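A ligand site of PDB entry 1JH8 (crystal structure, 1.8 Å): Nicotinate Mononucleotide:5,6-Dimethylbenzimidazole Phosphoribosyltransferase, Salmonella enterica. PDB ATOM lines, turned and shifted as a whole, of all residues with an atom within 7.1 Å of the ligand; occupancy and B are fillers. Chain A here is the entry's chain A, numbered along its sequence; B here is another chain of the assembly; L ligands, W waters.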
ATOM      1  N   SER A  80       0.282  23.578  -7.036  1.00  0.00           N
ATOM      2  CA  SER A  80       1.227  24.467  -6.353  1.00  0.00           C
ATOM      3  C   SER A  80       2.243  24.959  -7.384  1.00  0.00           C
ATOM      4  O   SER A  80       2.737  24.182  -8.189  1.00  0.00           O
ATOM      5  CB  SER A  80       2.011  23.754  -5.237  1.00  0.00           C
ATOM      6  OG  SER A  80       1.179  23.251  -4.202  1.00  0.00           O
ATOM      7  N   PRO A  81       2.584  26.243  -7.392  1.00  0.00           N
ATOM      8  CA  PRO A  81       3.591  26.679  -8.353  1.00  0.00           C
ATOM      9  C   PRO A  81       4.908  25.948  -8.084  1.00  0.00           C
ATOM     10  O   PRO A  81       5.223  25.630  -6.944  1.00  0.00           O
ATOM     11  CB  PRO A  81       3.742  28.184  -8.130  1.00  0.00           C
ATOM     12  CG  PRO A  81       2.552  28.638  -7.290  1.00  0.00           C
ATOM     13  CD  PRO A  81       1.902  27.391  -6.726  1.00  0.00           C
ATOM     14  N   VAL A  84       7.478  26.671  -5.194  1.00  0.00           N
ATOM     15  CA  VAL A  84       7.184  26.409  -3.806  1.00  0.00           C
ATOM     16  C   VAL A  84       8.192  25.454  -3.177  1.00  0.00           C
ATOM     17  O   VAL A  84       8.560  25.563  -2.023  1.00  0.00           O
ATOM     18  CB  VAL A  84       5.734  25.969  -3.601  1.00  0.00           C
ATOM     19  CG1 VAL A  84       5.500  25.603  -2.146  1.00  0.00           C
ATOM     20  CG2 VAL A  84       4.799  27.095  -4.019  1.00  0.00           C
ATOM     21  N   THR A  85       8.702  24.513  -3.968  1.00  0.00           N
ATOM     22  CA  THR A  85       9.698  23.586  -3.409  1.00  0.00           C
ATOM     23  C   THR A  85      10.903  24.339  -2.865  1.00  0.00           C
ATOM     24  O   THR A  85      11.388  24.118  -1.755  1.00  0.00           O
ATOM     25  CB  THR A  85      10.221  22.603  -4.465  1.00  0.00           C
ATOM     26  OG1 THR A  85       9.136  22.002  -5.167  1.00  0.00           O
ATOM     27  CG2 THR A  85      11.160  21.573  -3.803  1.00  0.00           C
ATOM     28  N   GLN A  88       9.907  26.688   0.179  1.00  0.00           N
ATOM     29  CA  GLN A  88       9.689  25.948   1.400  1.00  0.00           C
ATOM     30  C   GLN A  88      10.979  25.351   1.953  1.00  0.00           C
ATOM     31  O   GLN A  88      11.191  25.204   3.166  1.00  0.00           O
ATOM     32  CB  GLN A  88       8.595  24.884   1.188  1.00  0.00           C
ATOM     33  CG  GLN A  88       7.175  25.467   1.303  1.00  0.00           C
ATOM     34  CD  GLN A  88       6.873  25.913   2.743  1.00  0.00           C
ATOM     35  OE1 GLN A  88       7.466  26.896   3.224  1.00  0.00           O
ATOM     36  NE2 GLN A  88       5.947  25.203   3.418  1.00  0.00           N
ATOM     37  N   MET A  92      12.526  25.890   5.567  1.00  0.00           N
ATOM     38  CA  MET A  92      12.933  24.833   6.461  1.00  0.00           C
ATOM     39  C   MET A  92      14.133  25.316   7.251  1.00  0.00           C
ATOM     40  O   MET A  92      14.267  24.961   8.414  1.00  0.00           O
ATOM     41  CB  MET A  92      13.372  23.561   5.716  1.00  0.00           C
ATOM     42  CG  MET A  92      12.256  22.938   4.902  1.00  0.00           C
ATOM     43  SD  MET A  92      11.285  21.811   5.894  1.00  0.00           S
ATOM     44  CE  MET A  92      10.138  21.275   4.604  1.00  0.00           C
ATOM     45  N   THR A  97       8.396  26.023   9.000  1.00  0.00           N
ATOM     46  CA  THR A  97       7.497  25.042   8.391  1.00  0.00           C
ATOM     47  C   THR A  97       6.840  24.092   9.411  1.00  0.00           C
ATOM     48  O   THR A  97       7.234  23.984  10.600  1.00  0.00           O
ATOM     49  CB  THR A  97       8.192  24.196   7.300  1.00  0.00           C
ATOM     50  OG1 THR A  97       9.115  23.374   7.960  1.00  0.00           O
ATOM     51  CG2 THR A  97       8.872  25.062   6.241  1.00  0.00           C
ATOM     52  N   GLY A  98       5.853  23.373   8.898  1.00  0.00           N
ATOM     53  CA  GLY A  98       5.093  22.387   9.682  1.00  0.00           C
ATOM     54  C   GLY A  98       5.998  21.364  10.320  1.00  0.00           C
ATOM     55  O   GLY A  98       5.896  21.121  11.517  1.00  0.00           O
ATOM     56  N   GLU A 174       9.651  14.355   2.863  1.00  0.00           N
ATOM     57  CA  GLU A 174       9.960  14.873   1.541  1.00  0.00           C
ATOM     58  C   GLU A 174       9.285  16.212   1.341  1.00  0.00           C
ATOM     59  O   GLU A 174       8.382  16.580   2.073  1.00  0.00           O
ATOM     60  CB  GLU A 174       9.540  13.938   0.399  1.00  0.00           C
ATOM     61  CG  GLU A 174       8.132  13.384   0.647  1.00  0.00           C
ATOM     62  CD  GLU A 174       7.088  14.452   0.568  1.00  0.00           C
ATOM     63  OE1 GLU A 174       7.118  15.323  -0.275  1.00  0.00           O
ATOM     64  OE2 GLU A 174       6.164  14.362   1.509  1.00  0.00           O
ATOM     65  N   LEU A 175       9.751  16.895   0.301  1.00  0.00           N
ATOM     66  CA  LEU A 175       9.243  18.175  -0.130  1.00  0.00           C
ATOM     67  C   LEU A 175       9.474  18.255  -1.635  1.00  0.00           C
ATOM     68  O   LEU A 175      10.591  18.145  -2.117  1.00  0.00           O
ATOM     69  CB  LEU A 175       9.887  19.371   0.644  1.00  0.00           C
ATOM     70  CG  LEU A 175       9.433  20.749   0.196  1.00  0.00           C
ATOM     71  CD1 LEU A 175       8.028  21.023   0.746  1.00  0.00           C
ATOM     72  CD2 LEU A 175      10.423  21.810   0.700  1.00  0.00           C
ATOM     73  N   GLY A 176       8.395  18.387  -2.405  1.00  0.00           N
ATOM     74  CA  GLY A 176       8.554  18.452  -3.840  1.00  0.00           C
ATOM     75  C   GLY A 176       7.191  18.565  -4.495  1.00  0.00           C
ATOM     76  O   GLY A 176       6.348  17.696  -4.285  1.00  0.00           O
ATOM     77  N   MET A 177       6.983  19.639  -5.259  1.00  0.00           N
ATOM     78  CA  MET A 177       5.696  19.844  -5.933  1.00  0.00           C
ATOM     79  C   MET A 177       5.464  18.718  -6.945  1.00  0.00           C
ATOM     80  O   MET A 177       6.395  18.332  -7.675  1.00  0.00           O
ATOM     81  CB  MET A 177       5.639  21.223  -6.625  1.00  0.00           C
ATOM     82  CG  MET A 177       5.900  22.387  -5.669  1.00  0.00           C
ATOM     83  SD  MET A 177       4.853  22.365  -4.174  1.00  0.00           S
ATOM     84  CE  MET A 177       6.013  21.785  -2.890  1.00  0.00           C
ATOM     85  N   ALA A 178       4.233  18.220  -7.004  1.00  0.00           N
ATOM     86  CA  ALA A 178       3.879  17.132  -7.937  1.00  0.00           C
ATOM     87  C   ALA A 178       4.333  15.747  -7.481  1.00  0.00           C
ATOM     88  O   ALA A 178       4.216  14.753  -8.218  1.00  0.00           O
ATOM     89  CB  ALA A 178       4.376  17.392  -9.352  1.00  0.00           C
ATOM     90  N   ASN A 179       4.851  15.658  -6.260  1.00  0.00           N
ATOM     91  CA  ASN A 179       5.338  14.374  -5.757  1.00  0.00           C
ATOM     92  C   ASN A 179       4.367  13.208  -5.558  1.00  0.00           C
ATOM     93  O   ASN A 179       4.769  12.042  -5.552  1.00  0.00           O
ATOM     94  CB  ASN A 179       6.601  14.405  -4.870  1.00  0.00           C
ATOM     95  CG  ASN A 179       6.387  14.987  -3.491  1.00  0.00           C
ATOM     96  OD1 ASN A 179       5.202  15.261  -3.129  1.00  0.00           O
ATOM     97  ND2 ASN A 179       7.512  15.139  -2.744  1.00  0.00           N
ATOM     98  N   ALA A 203      -1.837  17.975  -2.969  1.00  0.00           N
ATOM     99  CA  ALA A 203      -1.995  19.302  -2.376  1.00  0.00           C
ATOM    100  C   ALA A 203      -3.163  20.054  -2.956  1.00  0.00           C
ATOM    101  O   ALA A 203      -2.997  20.999  -3.722  1.00  0.00           O
ATOM    102  CB  ALA A 203      -0.730  20.146  -2.409  1.00  0.00           C
ATOM    103  N   ARG A 314      -2.071  15.309   5.586  1.00  0.00           N
ATOM    104  CA  ARG A 314      -1.617  15.181   4.201  1.00  0.00           C
ATOM    105  C   ARG A 314      -0.657  16.311   3.842  1.00  0.00           C
ATOM    106  O   ARG A 314      -0.563  16.770   2.702  1.00  0.00           O
ATOM    107  CB  ARG A 314      -2.802  15.071   3.236  1.00  0.00           C
ATOM    108  CG  ARG A 314      -3.824  16.150   3.543  1.00  0.00           C
ATOM    109  CD  ARG A 314      -4.964  16.199   2.530  1.00  0.00           C
ATOM    110  NE  ARG A 314      -5.953  17.262   2.790  1.00  0.00           N
ATOM    111  CZ  ARG A 314      -5.928  18.496   2.276  1.00  0.00           C
ATOM    112  NH1 ARG A 314      -4.953  18.929   1.475  1.00  0.00           N
ATOM    113  NH2 ARG A 314      -6.929  19.330   2.595  1.00  0.00           N
ATOM    114  N   LEU A 315       0.109  16.763   4.821  1.00  0.00           N
ATOM    115  CA  LEU A 315       1.061  17.817   4.568  1.00  0.00           C
ATOM    116  C   LEU A 315       2.378  17.311   3.986  1.00  0.00           C
ATOM    117  O   LEU A 315       2.918  17.877   3.030  1.00  0.00           O
ATOM    118  CB  LEU A 315       1.291  18.710   5.806  1.00  0.00           C
ATOM    119  CG  LEU A 315       2.423  19.720   5.656  1.00  0.00           C
ATOM    120  CD1 LEU A 315       2.061  20.756   4.610  1.00  0.00           C
ATOM    121  CD2 LEU A 315       2.621  20.393   7.009  1.00  0.00           C
ATOM    122  N   GLY A 316       2.911  16.240   4.576  1.00  0.00           N
ATOM    123  CA  GLY A 316       4.188  15.719   4.157  1.00  0.00           C
ATOM    124  C   GLY A 316       5.265  16.375   5.006  1.00  0.00           C
ATOM    125  O   GLY A 316       5.018  16.743   6.185  1.00  0.00           O
ATOM    126  N   GLU A 317       6.465  16.507   4.419  1.00  0.00           N
ATOM    127  CA  GLU A 317       7.626  17.098   5.071  1.00  0.00           C
ATOM    128  C   GLU A 317       8.228  16.256   6.188  1.00  0.00           C
ATOM    129  O   GLU A 317       9.262  16.626   6.711  1.00  0.00           O
ATOM    130  CB  GLU A 317       7.298  18.460   5.735  1.00  0.00           C
ATOM    131  CG  GLU A 317       6.505  19.398   4.824  1.00  0.00           C
ATOM    132  CD  GLU A 317       6.401  20.750   5.458  1.00  0.00           C
ATOM    133  OE1 GLU A 317       6.790  20.994   6.581  1.00  0.00           O
ATOM    134  OE2 GLU A 317       5.857  21.636   4.667  1.00  0.00           O
ATOM    135  N   LEU B  29      -1.520  29.831   7.302  1.00  0.00           N
ATOM    136  CA  LEU B  29      -0.203  29.311   7.624  1.00  0.00           C
ATOM    137  C   LEU B  29       0.505  28.687   6.404  1.00  0.00           C
ATOM    138  O   LEU B  29      -0.130  28.337   5.421  1.00  0.00           O
ATOM    139  CB  LEU B  29      -0.298  28.279   8.756  1.00  0.00           C
ATOM    140  CG  LEU B  29      -0.276  28.801  10.183  1.00  0.00           C
ATOM    141  CD1 LEU B  29      -0.319  30.316  10.299  1.00  0.00           C
ATOM    142  CD2 LEU B  29      -1.366  28.109  10.993  1.00  0.00           C
ATOM    143  N   LEU B  30       1.826  28.532   6.517  1.00  0.00           N
ATOM    144  CA  LEU B  30       2.732  27.989   5.517  1.00  0.00           C
ATOM    145  C   LEU B  30       2.470  26.535   5.153  1.00  0.00           C
ATOM    146  O   LEU B  30       3.322  25.670   5.408  1.00  0.00           O
ATOM    147  CB  LEU B  30       4.123  28.079   6.158  1.00  0.00           C
ATOM    148  CG  LEU B  30       5.218  28.741   5.351  1.00  0.00           C
ATOM    149  CD1 LEU B  30       4.665  29.662   4.265  1.00  0.00           C
ATOM    150  CD2 LEU B  30       6.167  29.459   6.284  1.00  0.00           C
ATOM    151  N   LYS B  31       1.327  26.243   4.536  1.00  0.00           N
ATOM    152  CA  LYS B  31       0.968  24.878   4.167  1.00  0.00           C
ATOM    153  C   LYS B  31      -0.274  24.943   3.308  1.00  0.00           C
ATOM    154  O   LYS B  31      -0.986  25.949   3.365  1.00  0.00           O
ATOM    155  CB  LYS B  31       0.539  24.077   5.414  1.00  0.00           C
ATOM    156  CG  LYS B  31      -0.590  24.747   6.204  1.00  0.00           C
ATOM    157  CD  LYS B  31      -1.091  23.968   7.407  1.00  0.00           C
ATOM    158  CE  LYS B  31      -2.174  24.718   8.190  1.00  0.00           C
ATOM    159  NZ  LYS B  31      -3.407  24.934   7.415  1.00  0.00           N
ATOM    160  N   PRO B  32      -0.576  23.860   2.554  1.00  0.00           N
ATOM    161  CA  PRO B  32      -1.808  23.822   1.769  1.00  0.00           C
ATOM    162  C   PRO B  32      -2.963  23.804   2.763  1.00  0.00           C
ATOM    163  O   PRO B  32      -2.924  23.099   3.788  1.00  0.00           O
ATOM    164  CB  PRO B  32      -1.812  22.522   0.969  1.00  0.00           C
ATOM    165  CG  PRO B  32      -0.388  21.961   1.079  1.00  0.00           C
ATOM    166  CD  PRO B  32       0.323  22.719   2.181  1.00  0.00           C
ATOM    167  N   SER B  35      -4.392  20.911   5.087  1.00  0.00           N
ATOM    168  CA  SER B  35      -3.405  19.846   5.045  1.00  0.00           C
ATOM    169  C   SER B  35      -3.055  19.210   6.372  1.00  0.00           C
ATOM    170  O   SER B  35      -2.675  18.062   6.389  1.00  0.00           O
ATOM    171  CB  SER B  35      -2.164  20.181   4.252  1.00  0.00           C
ATOM    172  OG  SER B  35      -1.578  21.303   4.830  1.00  0.00           O
ATOM    173  N   LEU B 341       1.900  32.062   4.824  1.00  0.00           N
ATOM    174  CA  LEU B 341       2.021  32.013   3.382  1.00  0.00           C
ATOM    175  C   LEU B 341       2.332  33.369   2.758  1.00  0.00           C
ATOM    176  O   LEU B 341       3.175  33.504   1.856  1.00  0.00           O
ATOM    177  CB  LEU B 341       0.676  31.537   2.810  1.00  0.00           C
ATOM    178  CG  LEU B 341       0.491  30.037   2.897  1.00  0.00           C
ATOM    179  CD1 LEU B 341      -0.898  29.686   2.368  1.00  0.00           C
ATOM    180  CD2 LEU B 341       1.537  29.351   2.019  1.00  0.00           C
ATOM    181  N   ILE B 346       3.826  33.261  -1.155  1.00  0.00           N
ATOM    182  CA  ILE B 346       3.246  32.043  -1.681  1.00  0.00           C
ATOM    183  C   ILE B 346       1.741  32.196  -1.806  1.00  0.00           C
ATOM    184  O   ILE B 346       1.046  32.702  -0.924  1.00  0.00           O
ATOM    185  CB  ILE B 346       3.625  30.779  -0.905  1.00  0.00           C
ATOM    186  CG1 ILE B 346       5.119  30.539  -0.966  1.00  0.00           C
ATOM    187  CG2 ILE B 346       2.902  29.574  -1.491  1.00  0.00           C
ATOM    188  CD1 ILE B 346       5.672  29.773   0.232  1.00  0.00           C
ATOM    189  N   LEU B 348      -1.518  29.782  -2.793  1.00  0.00           N
ATOM    190  CA  LEU B 348      -2.083  28.469  -3.083  1.00  0.00           C
ATOM    191  C   LEU B 348      -3.603  28.501  -3.102  1.00  0.00           C
ATOM    192  O   LEU B 348      -4.243  29.111  -2.246  1.00  0.00           O
ATOM    193  CB  LEU B 348      -1.637  27.354  -2.102  1.00  0.00           C
ATOM    194  CG  LEU B 348      -0.134  27.289  -1.816  1.00  0.00           C
ATOM    195  CD1 LEU B 348       0.101  26.384  -0.603  1.00  0.00           C
ATOM    196  CD2 LEU B 348       0.619  26.739  -3.035  1.00  0.00           C
HETATM  197  N1  LIG L   1       4.767  21.417   2.415  1.00  0.00           N
HETATM  198  C1  LIG L   1       4.546  20.247   1.742  1.00  0.00           C
HETATM  199  N2  LIG L   1       3.843  20.399   0.599  1.00  0.00           N
HETATM  200  C2  LIG L   1       3.624  21.773   0.527  1.00  0.00           C
HETATM  201  C3  LIG L   1       2.954  22.585  -0.431  1.00  0.00           C
HETATM  202  N3  LIG L   1       2.370  22.167  -1.565  1.00  0.00           N
HETATM  203  N4  LIG L   1       2.883  23.918  -0.169  1.00  0.00           N
HETATM  204  C4  LIG L   1       3.482  24.388   0.970  1.00  0.00           C
HETATM  205  N5  LIG L   1       4.101  23.728   1.914  1.00  0.00           N
HETATM  206  C5  LIG L   1       4.160  22.408   1.635  1.00  0.00           C
HETATM  207  O   HOH W   1       3.168  19.408  -2.903  1.00  0.00           O
HETATM  208  O   HOH W   2       5.625  18.490  -1.267  1.00  0.00           O
HETATM  209  O   HOH W   3       5.552  17.453   1.101  1.00  0.00           O
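OE2 of Glu 317 lies within hydrogen-bond range of N1 of the ligand (2.5 Å). NE2 of Gln 88 is in hydrogen-bond range of N5 of the ligand, 2.8 Å away. The side-chain hydroxyl (OG) of Ser 80 is in hydrogen-bond range of a nitrogen (N3) of the ligand (3.1 Å). The side-chain sulfur of Met 177 lies within hydrogen-bond range of a nitrogen (N3) of the ligand (3.6 Å).
O of Glu 174 sits at hydrogen-bond distance from N of Glu 317 (3.0 Å). The side-chain carboxylate (OE1) of Glu 317 lies within hydrogen-bond range of the backbone NH (N) of Gly 98, at 3.5 Å. NE2 of Gln 88 is in hydrogen-bond range of O of Leu 30 of chain B, 3.3 Å away. The side-chain sulfur (SD) of Met 177 sits close to the side-chain hydroxyl (OG) of Ser 80, at 3.8 Å. N of Leu 315 lies within hydrogen-bond range of O of Ser 35 of chain B (3.4 Å). N of Met 177 lies within hydrogen-bond range of OG1 of Thr 85. O of Pro 32 of chain B sits at hydrogen-bond distance from OG of Ser 35 of chain B (2.5 Å).
CG1 of Val 84 touches N4 of the ligand, 3.7 Å away. Leu 175 touches the ligand. Ala 203 touches the ligand. O of Leu 315 touches C1 of the ligand, 3.2 Å away. Pro 32 of chain B touches the ligand (CD to N4, 3.7 Å). Leu 348 of chain B touches the ligand. Hydrophobic or aromatic side chains that line the ligand: Val 84, Leu 175, Met 177, Ala 203, Leu 315, Pro 32 of chain B and Leu 348 of chain B.
Water W3 lies within hydrogen-bond range of OE1 of Glu 174, O of Leu 315 and N2 of the ligand. Water W1 bridges a nitrogen (N3) of the ligand (3.2 Å) and the side-chain sulfur (SD) of Met 177 (3.6 Å). Water W2 bridges the backbone NH (N) of Gly 176 (3.0 Å) and a nitrogen (N2) of the ligand (3.2 Å).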
